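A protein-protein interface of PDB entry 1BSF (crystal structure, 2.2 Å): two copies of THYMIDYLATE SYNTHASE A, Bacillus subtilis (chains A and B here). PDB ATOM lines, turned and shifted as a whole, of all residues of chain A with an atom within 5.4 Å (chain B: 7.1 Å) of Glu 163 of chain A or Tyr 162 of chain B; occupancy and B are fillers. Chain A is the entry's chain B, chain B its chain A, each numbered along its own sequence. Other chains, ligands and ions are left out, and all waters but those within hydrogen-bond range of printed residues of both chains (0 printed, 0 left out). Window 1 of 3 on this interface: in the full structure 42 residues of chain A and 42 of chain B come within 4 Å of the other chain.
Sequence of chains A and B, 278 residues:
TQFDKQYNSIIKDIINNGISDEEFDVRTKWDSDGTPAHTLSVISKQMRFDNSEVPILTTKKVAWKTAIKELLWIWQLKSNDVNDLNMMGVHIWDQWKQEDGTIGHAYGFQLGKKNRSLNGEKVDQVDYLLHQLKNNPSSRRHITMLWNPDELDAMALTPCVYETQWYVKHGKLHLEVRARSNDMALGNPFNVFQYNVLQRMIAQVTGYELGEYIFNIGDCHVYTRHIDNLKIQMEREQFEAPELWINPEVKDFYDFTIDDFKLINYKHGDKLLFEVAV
Met 145 of chain A touches its own counterpart, Met 145 of chain B. Tyr 162 of chain A touches Glu 163 of chain B, and with the chains exchanged Glu 163 of chain A touches Tyr 162 of chain B. Glu 163 of chain A touches Arg 178 of chain B, but with the chains exchanged Arg 178 of chain A does not touch Glu 163 of chain B (4.1 Å). 9 positions are printed for both chains.
Among the printed residues, pairs that only touch across the chains: Met 145 of chain A with Trp 147 of chain B, Gln 165 of chain A with Arg 180 of chain B, Ile 143 of chain A with Arg 180 of chain B, Ile 143 of chain A with Trp 147 of chain B and Met 145 of chain A with Met 145 of chain B.
The backbone NH of Trp 147 of chain B sits close to the side-chain sulfur of Met 145 of chain B (3.6 Å). N of Leu 146 of chain B is in hydrogen-bond range of O of Tyr 162 of chain B. The backbone carbonyl oxygen (O) of Thr 158 of chain B lies within hydrogen-bond range of the guanidinium group (NH2) of Arg 180 of chain B (2.7 Å). OH of Tyr 162 of chain B is in hydrogen-bond range of NH1 of Arg 178 of chain B (2.5 Å). O of Tyr 162 of chain A sits at hydrogen-bond distance from N of Leu 146 of chain A (2.6 Å). The backbone carbonyl oxygen (O) of Gln 165 of chain A lies within hydrogen-bond range of the backbone NH (N) of Glu 176 of chain A.
The side-chain carboxylate (OE1) of Glu 163 of chain A is in hydrogen-bond range of the side-chain hydroxyl (OH) of Tyr 162 of chain B (2.6 Å). OH of Tyr 162 of chain A lies within hydrogen-bond range of OE1 of Glu 163 of chain B (2.7 Å). OE1 of Glu 163 of chain A lies within salt-bridge range of NH1 of Arg 178 of chain B (3.9 Å). The guanidinium group (NH2) of Arg 178 of chain B sits at hydrogen-bond distance from the side-chain amide oxygen (OE1) of Gln 165 of chain A, 2.9 Å away. NH2 of Arg 178 of chain B lies within salt-bridge range of OE1 of Glu 176 of chain A (2.8 Å).
Of the printed residues of chain B, Glu 163 of chain A touches Tyr 162 (2.6 Å) and Arg 178 (3.9 Å). Tyr 162 of chain B touches one residue of chain A. Printed residues of chain B within 4 Å of Tyr 162 of chain A: Glu 163 (2.7 Å). Of the printed residues of chain A, Arg 180 of chain B touches Ile 143 and Gln 165. Printed residues of chain B within 4 Å of Ile 143 of chain A: Trp 147 (3.9 Å) and Arg 180 (3.7 Å). Of the printed residues of chain A, Trp 147 of chain B touches Ile 143 and Met 145. Printed residues of chain B within 4 Å of Met 145 of chain A: Met 145 and Trp 147. The nearest residue of chain B that does not touch Glu 163 of chain A is Glu 163 of chain B (5.0 Å). The nearest residue of chain A that does not touch Tyr 162 of chain B is Met 145 of chain A (4.2 Å). The nearest printed residue of chain A that does not touch Trp 147 of chain B is Thr 144 of chain A (5.3 Å).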
ATOM      1  N   ILE A 143       6.239 -17.359  -9.145  1.00  0.00           N
ATOM      2  CA  ILE A 143       6.697 -16.141  -9.807  1.00  0.00           C
ATOM      3  C   ILE A 143       6.334 -15.994 -11.294  1.00  0.00           C
ATOM      4  O   ILE A 143       6.527 -16.918 -12.090  1.00  0.00           O
ATOM      5  CB  ILE A 143       8.238 -15.994  -9.692  1.00  0.00           C
ATOM      6  CG1 ILE A 143       8.682 -16.131  -8.234  1.00  0.00           C
ATOM      7  CG2 ILE A 143       8.679 -14.646 -10.246  1.00  0.00           C
ATOM      8  CD1 ILE A 143      10.178 -15.977  -8.064  1.00  0.00           C
ATOM      9  N   THR A 144       5.791 -14.830 -11.655  1.00  0.00           N
ATOM     10  CA  THR A 144       5.482 -14.528 -13.053  1.00  0.00           C
ATOM     11  C   THR A 144       6.586 -13.551 -13.438  1.00  0.00           C
ATOM     12  O   THR A 144       7.006 -12.704 -12.621  1.00  0.00           O
ATOM     13  CB  THR A 144       4.123 -13.838 -13.265  1.00  0.00           C
ATOM     14  OG1 THR A 144       4.329 -12.428 -13.389  1.00  0.00           O
ATOM     15  CG2 THR A 144       3.169 -14.131 -12.122  1.00  0.00           C
ATOM     16  N   MET A 145       7.048 -13.667 -14.680  1.00  0.00           N
ATOM     17  CA  MET A 145       8.156 -12.860 -15.167  1.00  0.00           C
ATOM     18  C   MET A 145       7.899 -12.324 -16.565  1.00  0.00           C
ATOM     19  O   MET A 145       7.694 -13.092 -17.500  1.00  0.00           O
ATOM     20  CB  MET A 145       9.427 -13.734 -15.135  1.00  0.00           C
ATOM     21  CG  MET A 145      10.724 -13.068 -15.587  1.00  0.00           C
ATOM     22  SD  MET A 145      10.976 -11.444 -14.869  1.00  0.00           S
ATOM     23  CE  MET A 145      10.851 -11.866 -13.149  1.00  0.00           C
ATOM     24  N   LEU A 146       7.892 -11.003 -16.717  1.00  0.00           N
ATOM     25  CA  LEU A 146       7.666 -10.409 -18.036  1.00  0.00           C
ATOM     26  C   LEU A 146       9.004 -10.130 -18.708  1.00  0.00           C
ATOM     27  O   LEU A 146       9.148 -10.309 -19.916  1.00  0.00           O
ATOM     28  CB  LEU A 146       6.852  -9.114 -17.926  1.00  0.00           C
ATOM     29  CG  LEU A 146       5.334  -9.292 -17.820  1.00  0.00           C
ATOM     30  CD1 LEU A 146       4.654  -7.950 -17.890  1.00  0.00           C
ATOM     31  CD2 LEU A 146       4.841 -10.204 -18.923  1.00  0.00           C
ATOM     32  N   VAL A 161       5.905  -2.867 -14.631  1.00  0.00           N
ATOM     33  CA  VAL A 161       5.554  -3.871 -13.644  1.00  0.00           C
ATOM     34  C   VAL A 161       5.737  -5.178 -14.406  1.00  0.00           C
ATOM     35  O   VAL A 161       4.842  -5.644 -15.117  1.00  0.00           O
ATOM     36  CB  VAL A 161       4.111  -3.675 -13.157  1.00  0.00           C
ATOM     37  CG1 VAL A 161       3.789  -4.647 -12.053  1.00  0.00           C
ATOM     38  CG2 VAL A 161       3.942  -2.259 -12.656  1.00  0.00           C
ATOM     39  N   TYR A 162       6.929  -5.749 -14.255  1.00  0.00           N
ATOM     40  CA  TYR A 162       7.332  -6.965 -14.956  1.00  0.00           C
ATOM     41  C   TYR A 162       7.258  -8.298 -14.212  1.00  0.00           C
ATOM     42  O   TYR A 162       7.244  -9.357 -14.843  1.00  0.00           O
ATOM     43  CB  TYR A 162       8.757  -6.778 -15.497  1.00  0.00           C
ATOM     44  CG  TYR A 162       9.824  -6.530 -14.437  1.00  0.00           C
ATOM     45  CD1 TYR A 162       9.761  -5.422 -13.582  1.00  0.00           C
ATOM     46  CD2 TYR A 162      10.910  -7.401 -14.299  1.00  0.00           C
ATOM     47  CE1 TYR A 162      10.769  -5.191 -12.609  1.00  0.00           C
ATOM     48  CE2 TYR A 162      11.913  -7.177 -13.336  1.00  0.00           C
ATOM     49  CZ  TYR A 162      11.839  -6.078 -12.499  1.00  0.00           C
ATOM     50  OH  TYR A 162      12.845  -5.873 -11.567  1.00  0.00           O
ATOM     51  N   GLU A 163       7.235  -8.262 -12.882  1.00  0.00           N
ATOM     52  CA  GLU A 163       7.163  -9.503 -12.121  1.00  0.00           C
ATOM     53  C   GLU A 163       6.278  -9.420 -10.892  1.00  0.00           C
ATOM     54  O   GLU A 163       5.791  -8.351 -10.514  1.00  0.00           O
ATOM     55  CB  GLU A 163       8.569  -9.983 -11.699  1.00  0.00           C
ATOM     56  CG  GLU A 163       9.441  -8.928 -11.012  1.00  0.00           C
ATOM     57  CD  GLU A 163       9.984  -9.365  -9.662  1.00  0.00           C
ATOM     58  OE1 GLU A 163      10.389 -10.541  -9.504  1.00  0.00           O
ATOM     59  OE2 GLU A 163      10.016  -8.513  -8.752  1.00  0.00           O
ATOM     60  N   THR A 164       6.073 -10.581 -10.281  1.00  0.00           N
ATOM     61  CA  THR A 164       5.270 -10.707  -9.077  1.00  0.00           C
ATOM     62  C   THR A 164       5.724 -11.959  -8.324  1.00  0.00           C
ATOM     63  O   THR A 164       6.273 -12.910  -8.915  1.00  0.00           O
ATOM     64  CB  THR A 164       3.753 -10.843  -9.397  1.00  0.00           C
ATOM     65  OG1 THR A 164       3.481 -12.161  -9.891  1.00  0.00           O
ATOM     66  CG2 THR A 164       3.323  -9.822 -10.448  1.00  0.00           C
ATOM     67  N   GLN A 165       5.522 -11.928  -7.012  1.00  0.00           N
ATOM     68  CA  GLN A 165       5.853 -13.052  -6.162  1.00  0.00           C
ATOM     69  C   GLN A 165       4.705 -13.181  -5.166  1.00  0.00           C
ATOM     70  O   GLN A 165       4.413 -12.246  -4.421  1.00  0.00           O
ATOM     71  CB  GLN A 165       7.173 -12.822  -5.412  1.00  0.00           C
ATOM     72  CG  GLN A 165       8.243 -13.832  -5.731  1.00  0.00           C
ATOM     73  CD  GLN A 165       9.074 -14.195  -4.538  1.00  0.00           C
ATOM     74  OE1 GLN A 165       9.889 -13.399  -4.067  1.00  0.00           O
ATOM     75  NE2 GLN A 165       8.883 -15.406  -4.035  1.00  0.00           N
ATOM     76  N   GLU A 176       3.405  -9.528  -3.882  1.00  0.00           N
ATOM     77  CA  GLU A 176       4.490  -8.560  -3.942  1.00  0.00           C
ATOM     78  C   GLU A 176       4.616  -8.223  -5.416  1.00  0.00           C
ATOM     79  O   GLU A 176       4.530  -9.111  -6.263  1.00  0.00           O
ATOM     80  CB  GLU A 176       5.804  -9.193  -3.442  1.00  0.00           C
ATOM     81  CG  GLU A 176       6.523  -8.419  -2.344  1.00  0.00           C
ATOM     82  CD  GLU A 176       7.925  -8.949  -2.059  1.00  0.00           C
ATOM     83  OE1 GLU A 176       8.203 -10.143  -2.327  1.00  0.00           O
ATOM     84  OE2 GLU A 176       8.759  -8.157  -1.558  1.00  0.00           O
ATOM     85  N   VAL A 177       4.832  -6.956  -5.732  1.00  0.00           N
ATOM     86  CA  VAL A 177       4.951  -6.558  -7.127  1.00  0.00           C
ATOM     87  C   VAL A 177       6.151  -5.639  -7.296  1.00  0.00           C
ATOM     88  O   VAL A 177       6.531  -4.941  -6.352  1.00  0.00           O
ATOM     89  CB  VAL A 177       3.686  -5.769  -7.606  1.00  0.00           C
ATOM     90  CG1 VAL A 177       3.843  -5.400  -9.053  1.00  0.00           C
ATOM     91  CG2 VAL A 177       2.413  -6.591  -7.401  1.00  0.00           C
ATOM     92  N   ARG A 178       6.748  -5.625  -8.487  1.00  0.00           N
ATOM     93  CA  ARG A 178       7.860  -4.713  -8.712  1.00  0.00           C
ATOM     94  C   ARG A 178       7.903  -4.026 -10.070  1.00  0.00           C
ATOM     95  O   ARG A 178       7.674  -4.642 -11.106  1.00  0.00           O
ATOM     96  CB  ARG A 178       9.212  -5.392  -8.459  1.00  0.00           C
ATOM     97  CG  ARG A 178      10.366  -4.396  -8.518  1.00  0.00           C
ATOM     98  CD  ARG A 178      11.394  -4.621  -7.414  1.00  0.00           C
ATOM     99  NE  ARG A 178      12.550  -3.728  -7.515  1.00  0.00           N
ATOM    100  CZ  ARG A 178      13.286  -3.555  -8.611  1.00  0.00           C
ATOM    101  NH1 ARG A 178      12.997  -4.203  -9.729  1.00  0.00           N
ATOM    102  NH2 ARG A 178      14.318  -2.717  -8.589  1.00  0.00           N
ATOM    103  N   TRP B  75      29.260 -14.839 -13.207  1.00  0.00           N
ATOM    104  CA  TRP B  75      29.371 -13.599 -13.977  1.00  0.00           C
ATOM    105  C   TRP B  75      30.632 -13.428 -14.824  1.00  0.00           C
ATOM    106  O   TRP B  75      30.605 -12.727 -15.827  1.00  0.00           O
ATOM    107  CB  TRP B  75      29.236 -12.391 -13.048  1.00  0.00           C
ATOM    108  CG  TRP B  75      27.919 -12.285 -12.349  1.00  0.00           C
ATOM    109  CD1 TRP B  75      27.543 -12.938 -11.213  1.00  0.00           C
ATOM    110  CD2 TRP B  75      26.840 -11.401 -12.678  1.00  0.00           C
ATOM    111  NE1 TRP B  75      26.300 -12.512 -10.804  1.00  0.00           N
ATOM    112  CE2 TRP B  75      25.845 -11.566 -11.686  1.00  0.00           C
ATOM    113  CE3 TRP B  75      26.618 -10.479 -13.713  1.00  0.00           C
ATOM    114  CZ2 TRP B  75      24.641 -10.845 -11.697  1.00  0.00           C
ATOM    115  CZ3 TRP B  75      25.415  -9.759 -13.724  1.00  0.00           C
ATOM    116  CH2 TRP B  75      24.445  -9.949 -12.720  1.00  0.00           C
ATOM    117  N   TYR B 107      21.875 -20.084 -13.980  1.00  0.00           N
ATOM    118  CA  TYR B 107      23.032 -19.299 -13.594  1.00  0.00           C
ATOM    119  C   TYR B 107      23.948 -18.813 -14.714  1.00  0.00           C
ATOM    120  O   TYR B 107      23.523 -18.034 -15.558  1.00  0.00           O
ATOM    121  CB  TYR B 107      23.800 -20.079 -12.536  1.00  0.00           C
ATOM    122  CG  TYR B 107      23.023 -20.160 -11.240  1.00  0.00           C
ATOM    123  CD1 TYR B 107      23.117 -19.143 -10.285  1.00  0.00           C
ATOM    124  CD2 TYR B 107      22.136 -21.208 -10.998  1.00  0.00           C
ATOM    125  CE1 TYR B 107      22.345 -19.162  -9.124  1.00  0.00           C
ATOM    126  CE2 TYR B 107      21.357 -21.236  -9.836  1.00  0.00           C
ATOM    127  CZ  TYR B 107      21.464 -20.209  -8.905  1.00  0.00           C
ATOM    128  OH  TYR B 107      20.690 -20.220  -7.763  1.00  0.00           O
ATOM    129  N   GLN B 125      23.949 -10.817 -21.914  1.00  0.00           N
ATOM    130  CA  GLN B 125      23.536  -9.939 -20.811  1.00  0.00           C
ATOM    131  C   GLN B 125      24.672  -9.159 -20.165  1.00  0.00           C
ATOM    132  O   GLN B 125      24.581  -7.942 -19.987  1.00  0.00           O
ATOM    133  CB  GLN B 125      22.854 -10.743 -19.706  1.00  0.00           C
ATOM    134  CG  GLN B 125      21.452 -11.184 -19.999  1.00  0.00           C
ATOM    135  CD  GLN B 125      20.677 -11.462 -18.733  1.00  0.00           C
ATOM    136  OE1 GLN B 125      20.441 -10.563 -17.929  1.00  0.00           O
ATOM    137  NE2 GLN B 125      20.281 -12.717 -18.543  1.00  0.00           N
ATOM    138  N   THR B 144      19.880  -7.347 -15.385  1.00  0.00           N
ATOM    139  CA  THR B 144      20.311  -8.710 -15.696  1.00  0.00           C
ATOM    140  C   THR B 144      19.187  -9.560 -15.115  1.00  0.00           C
ATOM    141  O   THR B 144      18.625  -9.235 -14.047  1.00  0.00           O
ATOM    142  CB  THR B 144      21.633  -9.123 -15.024  1.00  0.00           C
ATOM    143  OG1 THR B 144      21.342  -9.878 -13.844  1.00  0.00           O
ATOM    144  CG2 THR B 144      22.480  -7.913 -14.679  1.00  0.00           C
ATOM    145  N   MET B 145      18.867 -10.646 -15.814  1.00  0.00           N
ATOM    146  CA  MET B 145      17.762 -11.509 -15.429  1.00  0.00           C
ATOM    147  C   MET B 145      18.126 -12.981 -15.538  1.00  0.00           C
ATOM    148  O   MET B 145      18.481 -13.459 -16.610  1.00  0.00           O
ATOM    149  CB  MET B 145      16.560 -11.169 -16.335  1.00  0.00           C
ATOM    150  CG  MET B 145      15.273 -11.951 -16.081  1.00  0.00           C
ATOM    151  SD  MET B 145      14.833 -12.051 -14.346  1.00  0.00           S
ATOM    152  CE  MET B 145      14.808 -10.321 -13.953  1.00  0.00           C
ATOM    153  N   LEU B 146      18.055 -13.706 -14.425  1.00  0.00           N
ATOM    154  CA  LEU B 146      18.375 -15.135 -14.449  1.00  0.00           C
ATOM    155  C   LEU B 146      17.099 -15.942 -14.643  1.00  0.00           C
ATOM    156  O   LEU B 146      17.095 -16.948 -15.349  1.00  0.00           O
ATOM    157  CB  LEU B 146      19.081 -15.565 -13.158  1.00  0.00           C
ATOM    158  CG  LEU B 146      20.587 -15.296 -13.104  1.00  0.00           C
ATOM    159  CD1 LEU B 146      21.175 -15.916 -11.863  1.00  0.00           C
ATOM    160  CD2 LEU B 146      21.256 -15.842 -14.347  1.00  0.00           C
ATOM    161  N   TRP B 147      16.015 -15.477 -14.030  1.00  0.00           N
ATOM    162  CA  TRP B 147      14.709 -16.129 -14.133  1.00  0.00           C
ATOM    163  C   TRP B 147      14.179 -16.149 -15.571  1.00  0.00           C
ATOM    164  O   TRP B 147      13.429 -15.255 -15.975  1.00  0.00           O
ATOM    165  CB  TRP B 147      13.687 -15.414 -13.243  1.00  0.00           C
ATOM    166  CG  TRP B 147      12.505 -16.258 -12.924  1.00  0.00           C
ATOM    167  CD1 TRP B 147      11.307 -16.268 -13.576  1.00  0.00           C
ATOM    168  CD2 TRP B 147      12.395 -17.215 -11.864  1.00  0.00           C
ATOM    169  NE1 TRP B 147      10.455 -17.170 -12.986  1.00  0.00           N
ATOM    170  CE2 TRP B 147      11.096 -17.763 -11.933  1.00  0.00           C
ATOM    171  CE3 TRP B 147      13.268 -17.660 -10.862  1.00  0.00           C
ATOM    172  CZ2 TRP B 147      10.647 -18.737 -11.033  1.00  0.00           C
ATOM    173  CZ3 TRP B 147      12.821 -18.631  -9.966  1.00  0.00           C
ATOM    174  CH2 TRP B 147      11.521 -19.157 -10.059  1.00  0.00           C
ATOM    175  N   ASN B 148      14.569 -17.171 -16.333  1.00  0.00           N
ATOM    176  CA  ASN B 148      14.132 -17.322 -17.719  1.00  0.00           C
ATOM    177  C   ASN B 148      12.903 -18.217 -17.749  1.00  0.00           C
ATOM    178  O   ASN B 148      13.004 -19.427 -17.526  1.00  0.00           O
ATOM    179  CB  ASN B 148      15.226 -17.962 -18.563  1.00  0.00           C
ATOM    180  CG  ASN B 148      14.938 -17.890 -20.030  1.00  0.00           C
ATOM    181  OD1 ASN B 148      13.867 -17.437 -20.446  1.00  0.00           O
ATOM    182  ND2 ASN B 148      15.888 -18.332 -20.837  1.00  0.00           N
ATOM    183  N   THR B 158      16.271 -23.787  -9.426  1.00  0.00           N
ATOM    184  CA  THR B 158      15.770 -22.422  -9.532  1.00  0.00           C
ATOM    185  C   THR B 158      16.613 -21.440  -8.714  1.00  0.00           C
ATOM    186  O   THR B 158      16.717 -21.565  -7.495  1.00  0.00           O
ATOM    187  CB  THR B 158      14.324 -22.347  -9.037  1.00  0.00           C
ATOM    188  OG1 THR B 158      13.958 -23.611  -8.465  1.00  0.00           O
ATOM    189  CG2 THR B 158      13.385 -22.024 -10.185  1.00  0.00           C
ATOM    190  N   PRO B 159      17.185 -20.420  -9.374  1.00  0.00           N
ATOM    191  CA  PRO B 159      18.029 -19.401  -8.728  1.00  0.00           C
ATOM    192  C   PRO B 159      17.380 -18.507  -7.646  1.00  0.00           C
ATOM    193  O   PRO B 159      16.183 -18.214  -7.690  1.00  0.00           O
ATOM    194  CB  PRO B 159      18.566 -18.588  -9.909  1.00  0.00           C
ATOM    195  CG  PRO B 159      17.540 -18.779 -10.991  1.00  0.00           C
ATOM    196  CD  PRO B 159      17.022 -20.172 -10.819  1.00  0.00           C
ATOM    197  N   CYS B 160      18.194 -18.077  -6.682  1.00  0.00           N
ATOM    198  CA  CYS B 160      17.749 -17.215  -5.582  1.00  0.00           C
ATOM    199  C   CYS B 160      17.973 -15.768  -5.992  1.00  0.00           C
ATOM    200  O   CYS B 160      17.026 -15.023  -6.237  1.00  0.00           O
ATOM    201  CB  CYS B 160      18.553 -17.502  -4.307  1.00  0.00           C
ATOM    202  SG  CYS B 160      17.963 -18.895  -3.322  1.00  0.00           S
ATOM    203  N   VAL B 161      19.234 -15.359  -6.037  1.00  0.00           N
ATOM    204  CA  VAL B 161      19.551 -14.006  -6.460  1.00  0.00           C
ATOM    205  C   VAL B 161      19.540 -14.114  -7.980  1.00  0.00           C
ATOM    206  O   VAL B 161      20.536 -14.484  -8.609  1.00  0.00           O
ATOM    207  CB  VAL B 161      20.917 -13.570  -5.913  1.00  0.00           C
ATOM    208  CG1 VAL B 161      21.189 -12.130  -6.259  1.00  0.00           C
ATOM    209  CG2 VAL B 161      20.932 -13.744  -4.411  1.00  0.00           C
ATOM    210  N   TYR B 162      18.383 -13.798  -8.554  1.00  0.00           N
ATOM    211  CA  TYR B 162      18.141 -13.905  -9.990  1.00  0.00           C
ATOM    212  C   TYR B 162      18.230 -12.640 -10.844  1.00  0.00           C
ATOM    213  O   TYR B 162      18.386 -12.729 -12.064  1.00  0.00           O
ATOM    214  CB  TYR B 162      16.771 -14.560 -10.217  1.00  0.00           C
ATOM    215  CG  TYR B 162      15.585 -13.791  -9.648  1.00  0.00           C
ATOM    216  CD1 TYR B 162      15.479 -13.519  -8.277  1.00  0.00           C
ATOM    217  CD2 TYR B 162      14.554 -13.347 -10.482  1.00  0.00           C
ATOM    218  CE1 TYR B 162      14.362 -12.817  -7.755  1.00  0.00           C
ATOM    219  CE2 TYR B 162      13.442 -12.651  -9.970  1.00  0.00           C
ATOM    220  CZ  TYR B 162      13.351 -12.390  -8.615  1.00  0.00           C
ATOM    221  OH  TYR B 162      12.242 -11.712  -8.133  1.00  0.00           O
ATOM    222  N   GLU B 163      18.112 -11.469 -10.225  1.00  0.00           N
ATOM    223  CA  GLU B 163      18.191 -10.230 -10.990  1.00  0.00           C
ATOM    224  C   GLU B 163      18.935  -9.115 -10.279  1.00  0.00           C
ATOM    225  O   GLU B 163      19.303  -9.226  -9.106  1.00  0.00           O
ATOM    226  CB  GLU B 163      16.787  -9.726 -11.387  1.00  0.00           C
ATOM    227  CG  GLU B 163      15.775  -9.639 -10.241  1.00  0.00           C
ATOM    228  CD  GLU B 163      15.126  -8.273 -10.097  1.00  0.00           C
ATOM    229  OE1 GLU B 163      14.791  -7.632 -11.121  1.00  0.00           O
ATOM    230  OE2 GLU B 163      14.940  -7.843  -8.940  1.00  0.00           O
ATOM    231  N   THR B 164      19.157  -8.039 -11.024  1.00  0.00           N
ATOM    232  CA  THR B 164      19.835  -6.858 -10.520  1.00  0.00           C
ATOM    233  C   THR B 164      19.395  -5.654 -11.354  1.00  0.00           C
ATOM    234  O   THR B 164      18.979  -5.790 -12.523  1.00  0.00           O
ATOM    235  CB  THR B 164      21.384  -6.988 -10.615  1.00  0.00           C
ATOM    236  OG1 THR B 164      21.799  -6.823 -11.977  1.00  0.00           O
ATOM    237  CG2 THR B 164      21.849  -8.354 -10.119  1.00  0.00           C
ATOM    238  N   VAL B 177      19.656  -5.522  -5.658  1.00  0.00           N
ATOM    239  CA  VAL B 177      19.655  -6.952  -5.928  1.00  0.00           C
ATOM    240  C   VAL B 177      18.419  -7.589  -5.314  1.00  0.00           C
ATOM    241  O   VAL B 177      17.894  -7.082  -4.320  1.00  0.00           O
ATOM    242  CB  VAL B 177      20.906  -7.654  -5.296  1.00  0.00           C
ATOM    243  CG1 VAL B 177      20.875  -9.120  -5.620  1.00  0.00           C
ATOM    244  CG2 VAL B 177      22.205  -7.024  -5.799  1.00  0.00           C
ATOM    245  N   ARG B 178      17.949  -8.695  -5.890  1.00  0.00           N
ATOM    246  CA  ARG B 178      16.806  -9.373  -5.298  1.00  0.00           C
ATOM    247  C   ARG B 178      16.857 -10.894  -5.286  1.00  0.00           C
ATOM    248  O   ARG B 178      17.236 -11.529  -6.266  1.00  0.00           O
ATOM    249  CB  ARG B 178      15.486  -8.927  -5.941  1.00  0.00           C
ATOM    250  CG  ARG B 178      14.277  -9.498  -5.204  1.00  0.00           C
ATOM    251  CD  ARG B 178      13.158  -8.476  -5.034  1.00  0.00           C
ATOM    252  NE  ARG B 178      11.959  -9.037  -4.408  1.00  0.00           N
ATOM    253  CZ  ARG B 178      11.331 -10.139  -4.816  1.00  0.00           C
ATOM    254  NH1 ARG B 178      11.781 -10.829  -5.853  1.00  0.00           N
ATOM    255  NH2 ARG B 178      10.245 -10.557  -4.173  1.00  0.00           N
ATOM    256  N   ALA B 179      16.452 -11.460  -4.153  1.00  0.00           N
ATOM    257  CA  ALA B 179      16.410 -12.907  -3.939  1.00  0.00           C
ATOM    258  C   ALA B 179      14.948 -13.358  -3.759  1.00  0.00           C
ATOM    259  O   ALA B 179      14.197 -12.736  -3.012  1.00  0.00           O
ATOM    260  CB  ALA B 179      17.237 -13.264  -2.682  1.00  0.00           C
ATOM    261  N   ARG B 180      14.533 -14.423  -4.439  1.00  0.00           N
ATOM    262  CA  ARG B 180      13.155 -14.884  -4.269  1.00  0.00           C
ATOM    263  C   ARG B 180      13.035 -15.597  -2.923  1.00  0.00           C
ATOM    264  O   ARG B 180      11.951 -15.745  -2.370  1.00  0.00           O
ATOM    265  CB  ARG B 180      12.716 -15.817  -5.407  1.00  0.00           C
ATOM    266  CG  ARG B 180      13.801 -16.714  -5.988  1.00  0.00           C
ATOM    267  CD  ARG B 180      13.263 -18.114  -6.296  1.00  0.00           C
ATOM    268  NE  ARG B 180      14.291 -19.138  -6.137  1.00  0.00           N
ATOM    269  CZ  ARG B 180      14.146 -20.244  -5.411  1.00  0.00           C
ATOM    270  NH1 ARG B 180      13.008 -20.479  -4.776  1.00  0.00           N
ATOM    271  NH2 ARG B 180      15.138 -21.118  -5.325  1.00  0.00           N
ATOM    272  N   SER B 181      14.165 -16.039  -2.400  1.00  0.00           N
ATOM    273  CA  SER B 181      14.197 -16.705  -1.108  1.00  0.00           C
ATOM    274  C   SER B 181      15.583 -16.461  -0.549  1.00  0.00           C
ATOM    275  O   SER B 181      16.460 -15.962  -1.256  1.00  0.00           O
ATOM    276  CB  SER B 181      13.950 -18.211  -1.248  1.00  0.00           C
ATOM    277  OG  SER B 181      13.585 -18.781   0.001  1.00  0.00           O
ATOM    278  N   TYR B 195      27.412 -10.251  -3.733  1.00  0.00           N
ATOM    279  CA  TYR B 195      26.908  -9.436  -4.837  1.00  0.00           C
ATOM    280  C   TYR B 195      27.333  -7.984  -4.705  1.00  0.00           C
ATOM    281  O   TYR B 195      27.110  -7.182  -5.613  1.00  0.00           O
ATOM    282  CB  TYR B 195      25.386  -9.570  -4.963  1.00  0.00           C
ATOM    283  CG  TYR B 195      24.975 -10.632  -5.973  1.00  0.00           C
ATOM    284  CD1 TYR B 195      24.877 -11.974  -5.603  1.00  0.00           C
ATOM    285  CD2 TYR B 195      24.717 -10.304  -7.308  1.00  0.00           C
ATOM    286  CE1 TYR B 195      24.527 -12.971  -6.546  1.00  0.00           C
ATOM    287  CE2 TYR B 195      24.367 -11.300  -8.262  1.00  0.00           C
ATOM    288  CZ  TYR B 195      24.274 -12.619  -7.866  1.00  0.00           C
ATOM    289  OH  TYR B 195      23.903 -13.585  -8.770  1.00  0.00           O
ATOM    290  N   ASN B 216      17.474  -7.061  -1.789  1.00  0.00           N
ATOM    291  CA  ASN B 216      16.091  -7.432  -1.518  1.00  0.00           C
ATOM    292  C   ASN B 216      15.848  -8.930  -1.419  1.00  0.00           C
ATOM    293  O   ASN B 216      16.285  -9.720  -2.269  1.00  0.00           O
ATOM    294  CB  ASN B 216      15.161  -6.817  -2.575  1.00  0.00           C
ATOM    295  CG  ASN B 216      15.294  -5.321  -2.647  1.00  0.00           C
ATOM    296  OD1 ASN B 216      15.275  -4.653  -1.629  1.00  0.00           O
ATOM    297  ND2 ASN B 216      15.450  -4.789  -3.847  1.00  0.00           N
